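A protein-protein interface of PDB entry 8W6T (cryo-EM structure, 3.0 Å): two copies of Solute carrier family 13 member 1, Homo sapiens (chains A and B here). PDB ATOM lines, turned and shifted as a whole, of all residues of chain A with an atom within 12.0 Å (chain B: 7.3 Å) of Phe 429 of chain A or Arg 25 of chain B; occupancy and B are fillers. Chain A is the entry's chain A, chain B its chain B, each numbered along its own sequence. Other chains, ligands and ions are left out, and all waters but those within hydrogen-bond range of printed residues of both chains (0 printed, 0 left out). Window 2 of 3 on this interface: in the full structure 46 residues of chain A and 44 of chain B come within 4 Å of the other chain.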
ATOM      1  N   PHE A 410      -0.488 -22.068 -27.103  1.00  0.00           N
ATOM      2  CA  PHE A 410      -0.245 -21.138 -28.197  1.00  0.00           C
ATOM      3  C   PHE A 410      -1.394 -20.163 -28.407  1.00  0.00           C
ATOM      4  O   PHE A 410      -1.231 -19.191 -29.153  1.00  0.00           O
ATOM      5  CB  PHE A 410       0.009 -21.913 -29.496  1.00  0.00           C
ATOM      6  CG  PHE A 410       1.180 -22.853 -29.427  1.00  0.00           C
ATOM      7  CD1 PHE A 410       2.451 -22.418 -29.763  1.00  0.00           C
ATOM      8  CD2 PHE A 410       1.008 -24.176 -29.049  1.00  0.00           C
ATOM      9  CE1 PHE A 410       3.533 -23.273 -29.692  1.00  0.00           C
ATOM     10  CE2 PHE A 410       2.085 -25.040 -28.988  1.00  0.00           C
ATOM     11  CZ  PHE A 410       3.348 -24.587 -29.312  1.00  0.00           C
ATOM     12  N   LEU A 411      -2.539 -20.391 -27.769  1.00  0.00           N
ATOM     13  CA  LEU A 411      -3.745 -19.598 -27.970  1.00  0.00           C
ATOM     14  C   LEU A 411      -4.091 -18.679 -26.813  1.00  0.00           C
ATOM     15  O   LEU A 411      -4.552 -17.562 -27.047  1.00  0.00           O
ATOM     16  CB  LEU A 411      -4.941 -20.518 -28.230  1.00  0.00           C
ATOM     17  CG  LEU A 411      -5.296 -20.738 -29.692  1.00  0.00           C
ATOM     18  CD1 LEU A 411      -6.340 -21.826 -29.820  1.00  0.00           C
ATOM     19  CD2 LEU A 411      -5.805 -19.430 -30.259  1.00  0.00           C
ATOM     20  N   ILE A 412      -3.906 -19.128 -25.579  1.00  0.00           N
ATOM     21  CA  ILE A 412      -4.402 -18.380 -24.417  1.00  0.00           C
ATOM     22  C   ILE A 412      -3.528 -17.150 -24.197  1.00  0.00           C
ATOM     23  O   ILE A 412      -2.290 -17.267 -24.200  1.00  0.00           O
ATOM     24  CB  ILE A 412      -4.430 -19.281 -23.179  1.00  0.00           C
ATOM     25  CG1 ILE A 412      -5.459 -20.395 -23.374  1.00  0.00           C
ATOM     26  CG2 ILE A 412      -4.770 -18.489 -21.929  1.00  0.00           C
ATOM     27  CD1 ILE A 412      -5.458 -21.429 -22.281  1.00  0.00           C
ATOM     28  N   PRO A 413      -4.115 -15.959 -24.058  1.00  0.00           N
ATOM     29  CA  PRO A 413      -3.309 -14.745 -23.881  1.00  0.00           C
ATOM     30  C   PRO A 413      -2.577 -14.718 -22.548  1.00  0.00           C
ATOM     31  O   PRO A 413      -3.062 -15.229 -21.536  1.00  0.00           O
ATOM     32  CB  PRO A 413      -4.345 -13.616 -23.960  1.00  0.00           C
ATOM     33  CG  PRO A 413      -5.670 -14.270 -23.818  1.00  0.00           C
ATOM     34  CD  PRO A 413      -5.522 -15.645 -24.351  1.00  0.00           C
ATOM     35  N   ALA A 414      -1.392 -14.117 -22.563  1.00  0.00           N
ATOM     36  CA  ALA A 414      -0.589 -13.940 -21.363  1.00  0.00           C
ATOM     37  C   ALA A 414      -0.305 -12.483 -21.039  1.00  0.00           C
ATOM     38  O   ALA A 414      -0.524 -12.057 -19.904  1.00  0.00           O
ATOM     39  CB  ALA A 414       0.737 -14.699 -21.505  1.00  0.00           C
ATOM     40  N   LYS A 415       0.166 -11.702 -22.010  1.00  0.00           N
ATOM     41  CA  LYS A 415       0.547 -10.314 -21.771  1.00  0.00           C
ATOM     42  C   LYS A 415       0.134  -9.471 -22.967  1.00  0.00           C
ATOM     43  O   LYS A 415       0.282  -9.906 -24.112  1.00  0.00           O
ATOM     44  CB  LYS A 415       2.058 -10.187 -21.530  1.00  0.00           C
ATOM     45  CG  LYS A 415       2.532 -10.652 -20.157  1.00  0.00           C
ATOM     46  CD  LYS A 415       4.029 -10.478 -19.996  1.00  0.00           C
ATOM     47  CE  LYS A 415       4.498 -10.970 -18.641  1.00  0.00           C
ATOM     48  NZ  LYS A 415       5.972 -10.822 -18.483  1.00  0.00           N
ATOM     49  N   THR A 416      -0.382  -8.275 -22.701  1.00  0.00           N
ATOM     50  CA  THR A 416      -0.720  -7.355 -23.774  1.00  0.00           C
ATOM     51  C   THR A 416       0.533  -6.671 -24.309  1.00  0.00           C
ATOM     52  O   THR A 416       1.603  -6.699 -23.697  1.00  0.00           O
ATOM     53  CB  THR A 416      -1.717  -6.302 -23.292  1.00  0.00           C
ATOM     54  OG1 THR A 416      -1.170  -5.607 -22.166  1.00  0.00           O
ATOM     55  CG2 THR A 416      -3.027  -6.953 -22.889  1.00  0.00           C
ATOM     56  N   LEU A 417       0.388  -6.048 -25.473  1.00  0.00           N
ATOM     57  CA  LEU A 417       1.501  -5.368 -26.123  1.00  0.00           C
ATOM     58  C   LEU A 417       1.187  -3.893 -26.350  1.00  0.00           C
ATOM     59  O   LEU A 417       1.924  -3.013 -25.904  1.00  0.00           O
ATOM     60  CB  LEU A 417       1.840  -6.044 -27.453  1.00  0.00           C
ATOM     61  CG  LEU A 417       2.955  -7.092 -27.439  1.00  0.00           C
ATOM     62  CD1 LEU A 417       2.472  -8.387 -26.831  1.00  0.00           C
ATOM     63  CD2 LEU A 417       3.479  -7.330 -28.844  1.00  0.00           C
ATOM     64  N   PHE A 429      -0.518  -3.273 -31.208  1.00  0.00           N
ATOM     65  CA  PHE A 429      -1.161  -3.312 -29.901  1.00  0.00           C
ATOM     66  C   PHE A 429      -1.883  -4.649 -29.744  1.00  0.00           C
ATOM     67  O   PHE A 429      -3.094  -4.705 -29.550  1.00  0.00           O
ATOM     68  CB  PHE A 429      -2.124  -2.136 -29.743  1.00  0.00           C
ATOM     69  CG  PHE A 429      -2.438  -1.796 -28.317  1.00  0.00           C
ATOM     70  CD1 PHE A 429      -1.467  -1.248 -27.495  1.00  0.00           C
ATOM     71  CD2 PHE A 429      -3.703  -2.003 -27.804  1.00  0.00           C
ATOM     72  CE1 PHE A 429      -1.751  -0.928 -26.180  1.00  0.00           C
ATOM     73  CE2 PHE A 429      -3.996  -1.687 -26.490  1.00  0.00           C
ATOM     74  CZ  PHE A 429      -3.019  -1.147 -25.679  1.00  0.00           C
ATOM     75  N   ASP A 430      -1.102  -5.721 -29.834  1.00  0.00           N
ATOM     76  CA  ASP A 430      -1.580  -7.094 -29.860  1.00  0.00           C
ATOM     77  C   ASP A 430      -1.618  -7.676 -28.447  1.00  0.00           C
ATOM     78  O   ASP A 430      -1.539  -6.958 -27.448  1.00  0.00           O
ATOM     79  CB  ASP A 430      -0.685  -7.924 -30.775  1.00  0.00           C
ATOM     80  CG  ASP A 430      -1.454  -8.938 -31.583  1.00  0.00           C
ATOM     81  OD1 ASP A 430      -2.631  -9.200 -31.261  1.00  0.00           O
ATOM     82  OD2 ASP A 430      -0.870  -9.476 -32.545  1.00  0.00           O
ATOM     83  N   TYR A 431      -1.774  -8.994 -28.355  1.00  0.00           N
ATOM     84  CA  TYR A 431      -1.523  -9.758 -27.142  1.00  0.00           C
ATOM     85  C   TYR A 431      -0.320 -10.670 -27.379  1.00  0.00           C
ATOM     86  O   TYR A 431       0.211 -10.763 -28.487  1.00  0.00           O
ATOM     87  CB  TYR A 431      -2.768 -10.555 -26.719  1.00  0.00           C
ATOM     88  CG  TYR A 431      -3.043 -11.825 -27.509  1.00  0.00           C
ATOM     89  CD1 TYR A 431      -3.765 -11.787 -28.691  1.00  0.00           C
ATOM     90  CD2 TYR A 431      -2.611 -13.067 -27.049  1.00  0.00           C
ATOM     91  CE1 TYR A 431      -4.021 -12.942 -29.407  1.00  0.00           C
ATOM     92  CE2 TYR A 431      -2.857 -14.218 -27.757  1.00  0.00           C
ATOM     93  CZ  TYR A 431      -3.558 -14.152 -28.933  1.00  0.00           C
ATOM     94  OH  TYR A 431      -3.809 -15.310 -29.629  1.00  0.00           O
ATOM     95  N   SER A 432       0.105 -11.356 -26.319  1.00  0.00           N
ATOM     96  CA  SER A 432       1.151 -12.361 -26.414  1.00  0.00           C
ATOM     97  C   SER A 432       0.604 -13.677 -25.868  1.00  0.00           C
ATOM     98  O   SER A 432      -0.142 -13.669 -24.876  1.00  0.00           O
ATOM     99  CB  SER A 432       2.404 -11.943 -25.640  1.00  0.00           C
ATOM    100  OG  SER A 432       3.402 -12.943 -25.710  1.00  0.00           O
ATOM    101  N   PRO A 433       0.937 -14.816 -26.482  1.00  0.00           N
ATOM    102  CA  PRO A 433       0.457 -16.100 -25.957  1.00  0.00           C
ATOM    103  C   PRO A 433       1.312 -16.602 -24.806  1.00  0.00           C
ATOM    104  O   PRO A 433       2.226 -15.907 -24.353  1.00  0.00           O
ATOM    105  CB  PRO A 433       0.549 -17.022 -27.176  1.00  0.00           C
ATOM    106  CG  PRO A 433       1.694 -16.480 -27.941  1.00  0.00           C
ATOM    107  CD  PRO A 433       1.671 -14.984 -27.748  1.00  0.00           C
ATOM    108  N   LEU B  21     -14.938  -2.469 -27.333  1.00  0.00           N
ATOM    109  CA  LEU B  21     -13.905  -1.682 -27.996  1.00  0.00           C
ATOM    110  C   LEU B  21     -12.550  -2.378 -27.912  1.00  0.00           C
ATOM    111  O   LEU B  21     -11.573  -1.920 -28.500  1.00  0.00           O
ATOM    112  CB  LEU B  21     -13.807  -0.277 -27.387  1.00  0.00           C
ATOM    113  CG  LEU B  21     -14.870   0.785 -27.707  1.00  0.00           C
ATOM    114  CD1 LEU B  21     -16.136   0.633 -26.866  1.00  0.00           C
ATOM    115  CD2 LEU B  21     -14.290   2.184 -27.547  1.00  0.00           C
ATOM    116  N   VAL B  22     -12.500  -3.492 -27.182  1.00  0.00           N
ATOM    117  CA  VAL B  22     -11.271  -4.242 -26.961  1.00  0.00           C
ATOM    118  C   VAL B  22     -11.190  -5.481 -27.844  1.00  0.00           C
ATOM    119  O   VAL B  22     -10.436  -6.410 -27.535  1.00  0.00           O
ATOM    120  CB  VAL B  22     -11.104  -4.615 -25.478  1.00  0.00           C
ATOM    121  CG1 VAL B  22     -10.928  -3.364 -24.638  1.00  0.00           C
ATOM    122  CG2 VAL B  22     -12.307  -5.410 -24.992  1.00  0.00           C
ATOM    123  N   TYR B  23     -11.941  -5.519 -28.942  1.00  0.00           N
ATOM    124  CA  TYR B  23     -11.889  -6.646 -29.861  1.00  0.00           C
ATOM    125  C   TYR B  23     -10.654  -6.633 -30.752  1.00  0.00           C
ATOM    126  O   TYR B  23     -10.210  -7.703 -31.181  1.00  0.00           O
ATOM    127  CB  TYR B  23     -13.145  -6.672 -30.736  1.00  0.00           C
ATOM    128  CG  TYR B  23     -14.430  -6.480 -29.969  1.00  0.00           C
ATOM    129  CD1 TYR B  23     -14.907  -7.470 -29.120  1.00  0.00           C
ATOM    130  CD2 TYR B  23     -15.166  -5.309 -30.093  1.00  0.00           C
ATOM    131  CE1 TYR B  23     -16.085  -7.300 -28.412  1.00  0.00           C
ATOM    132  CE2 TYR B  23     -16.345  -5.128 -29.391  1.00  0.00           C
ATOM    133  CZ  TYR B  23     -16.799  -6.126 -28.553  1.00  0.00           C
ATOM    134  OH  TYR B  23     -17.972  -5.952 -27.853  1.00  0.00           O
ATOM    135  N   ARG B  24     -10.085  -5.461 -31.033  1.00  0.00           N
ATOM    136  CA  ARG B  24      -8.935  -5.368 -31.922  1.00  0.00           C
ATOM    137  C   ARG B  24      -7.625  -5.746 -31.245  1.00  0.00           C
ATOM    138  O   ARG B  24      -6.605  -5.882 -31.932  1.00  0.00           O
ATOM    139  CB  ARG B  24      -8.820  -3.951 -32.494  1.00  0.00           C
ATOM    140  CG  ARG B  24      -8.395  -3.908 -33.955  1.00  0.00           C
ATOM    141  CD  ARG B  24      -9.369  -4.678 -34.837  1.00  0.00           C
ATOM    142  NE  ARG B  24      -8.870  -4.847 -36.200  1.00  0.00           N
ATOM    143  CZ  ARG B  24      -9.485  -5.560 -37.139  1.00  0.00           C
ATOM    144  NH1 ARG B  24     -10.630  -6.172 -36.868  1.00  0.00           N
ATOM    145  NH2 ARG B  24      -8.957  -5.659 -38.351  1.00  0.00           N
ATOM    146  N   ARG B  25      -7.625  -5.915 -29.922  1.00  0.00           N
ATOM    147  CA  ARG B  25      -6.428  -6.366 -29.221  1.00  0.00           C
ATOM    148  C   ARG B  25      -6.287  -7.879 -29.316  1.00  0.00           C
ATOM    149  O   ARG B  25      -5.338  -8.392 -29.917  1.00  0.00           O
ATOM    150  CB  ARG B  25      -6.481  -5.930 -27.754  1.00  0.00           C
ATOM    151  CG  ARG B  25      -6.263  -4.449 -27.523  1.00  0.00           C
ATOM    152  CD  ARG B  25      -7.564  -3.656 -27.466  1.00  0.00           C
ATOM    153  NE  ARG B  25      -7.350  -2.303 -26.960  1.00  0.00           N
ATOM    154  CZ  ARG B  25      -8.210  -1.300 -27.110  1.00  0.00           C
ATOM    155  NH1 ARG B  25      -7.931  -0.104 -26.614  1.00  0.00           N
ATOM    156  NH2 ARG B  25      -9.346  -1.493 -27.763  1.00  0.00           N
ATOM    157  N   PHE B  26      -7.243  -8.606 -28.740  1.00  0.00           N
ATOM    158  CA  PHE B  26      -7.313 -10.059 -28.863  1.00  0.00           C
ATOM    159  C   PHE B  26      -8.064 -10.361 -30.153  1.00  0.00           C
ATOM    160  O   PHE B  26      -9.262 -10.653 -30.171  1.00  0.00           O
ATOM    161  CB  PHE B  26      -7.984 -10.665 -27.640  1.00  0.00           C
ATOM    162  CG  PHE B  26      -7.568 -10.021 -26.353  1.00  0.00           C
ATOM    163  CD1 PHE B  26      -6.292 -10.217 -25.851  1.00  0.00           C
ATOM    164  CD2 PHE B  26      -8.443  -9.207 -25.655  1.00  0.00           C
ATOM    165  CE1 PHE B  26      -5.898  -9.621 -24.668  1.00  0.00           C
ATOM    166  CE2 PHE B  26      -8.058  -8.608 -24.471  1.00  0.00           C
ATOM    167  CZ  PHE B  26      -6.783  -8.816 -23.977  1.00  0.00           C
ATOM    168  N   LEU B  27      -7.328 -10.275 -31.258  1.00  0.00           N
ATOM    169  CA  LEU B  27      -7.947 -10.257 -32.577  1.00  0.00           C
ATOM    170  C   LEU B  27      -7.972 -11.650 -33.192  1.00  0.00           C
ATOM    171  O   LEU B  27      -8.964 -12.047 -33.808  1.00  0.00           O
ATOM    172  CB  LEU B  27      -7.201  -9.271 -33.477  1.00  0.00           C
ATOM    173  CG  LEU B  27      -7.793  -8.993 -34.851  1.00  0.00           C
ATOM    174  CD1 LEU B  27      -9.184  -8.421 -34.678  1.00  0.00           C
ATOM    175  CD2 LEU B  27      -6.899  -8.026 -35.605  1.00  0.00           C
ATOM    176  N   PHE B  28      -6.886 -12.403 -33.041  1.00  0.00           N
ATOM    177  CA  PHE B  28      -6.858 -13.797 -33.474  1.00  0.00           C
ATOM    178  C   PHE B  28      -7.010 -14.756 -32.302  1.00  0.00           C
ATOM    179  O   PHE B  28      -6.473 -15.863 -32.319  1.00  0.00           O
ATOM    180  CB  PHE B  28      -5.601 -14.110 -34.289  1.00  0.00           C
ATOM    181  CG  PHE B  28      -4.308 -13.677 -33.655  1.00  0.00           C
ATOM    182  CD1 PHE B  28      -3.584 -14.552 -32.860  1.00  0.00           C
ATOM    183  CD2 PHE B  28      -3.781 -12.421 -33.908  1.00  0.00           C
ATOM    184  CE1 PHE B  28      -2.382 -14.166 -32.296  1.00  0.00           C
ATOM    185  CE2 PHE B  28      -2.585 -12.031 -33.343  1.00  0.00           C
ATOM    186  CZ  PHE B  28      -1.884 -12.904 -32.537  1.00  0.00           C
ATOM    187  N   VAL B  29      -7.715 -14.339 -31.259  1.00  0.00           N
ATOM    188  CA  VAL B  29      -8.381 -15.259 -30.343  1.00  0.00           C
ATOM    189  C   VAL B  29      -9.831 -15.453 -30.749  1.00  0.00           C
ATOM    190  O   VAL B  29     -10.296 -16.580 -30.913  1.00  0.00           O
ATOM    191  CB  VAL B  29      -8.269 -14.759 -28.884  1.00  0.00           C
ATOM    192  CG1 VAL B  29      -9.270 -15.469 -27.980  1.00  0.00           C
ATOM    193  CG2 VAL B  29      -6.885 -14.998 -28.359  1.00  0.00           C
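Printed residues of chain B within 4 Å of Phe 429 of chain A: Arg 25. Of the printed residues of chain B, Asp 430 of chain A touches Arg 25 (3.1 Å) and Phe 28 (3.2 Å). Of the printed residues of chain B, Tyr 431 of chain A touches Arg 25 (3.9 Å), Phe 26 (3.6 Å), Phe 28 (3.2 Å) and Val 29 (3.3 Å). No residue of chain A comes within 4 Å of Leu 21 of chain B. No residue of chain A comes within 4 Å of Val 22 of chain B. Arg 25 of chain B touches just these residues of chain A: Phe 429, Asp 430 and Tyr 431. Of the printed residues of chain A, Phe 26 of chain B touches Tyr 431 (3.6 Å). No residue of chain A comes within 4 Å of Leu 27 of chain B. Phe 28 of chain B touches two residues of chain A. Of the printed residues of chain A, Val 29 of chain B touches Leu 411 (3.7 Å) and Tyr 431 (3.3 Å). The nearest residue of chain B that does not touch Phe 429 of chain A is Arg 24 of chain B (4.4 Å).
Of the 13 printed residues of chain A, 4 touch a printed residue of chain B.
No position is printed for both chains.
O of Arg 25 of chain B lies close to OD1 of Asp 430 of chain A (3.1 Å).
Among the printed residues, merely in contact across the chains: Asp 430 of chain A with Phe 28 of chain B, Tyr 431 of chain A with Phe 28 of chain B, Tyr 431 of chain A with Val 29 of chain B, Phe 429 of chain A with Arg 25 of chain B, Tyr 431 of chain A with Phe 26 of chain B, Leu 411 of chain A with Val 29 of chain B and Tyr 431 of chain A with Arg 25 of chain B.
The backbone NH (N) of Leu 417 of chain A lies within hydrogen-bond range of the backbone carbonyl oxygen (O) of Asp 430 of chain A (2.9 Å).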
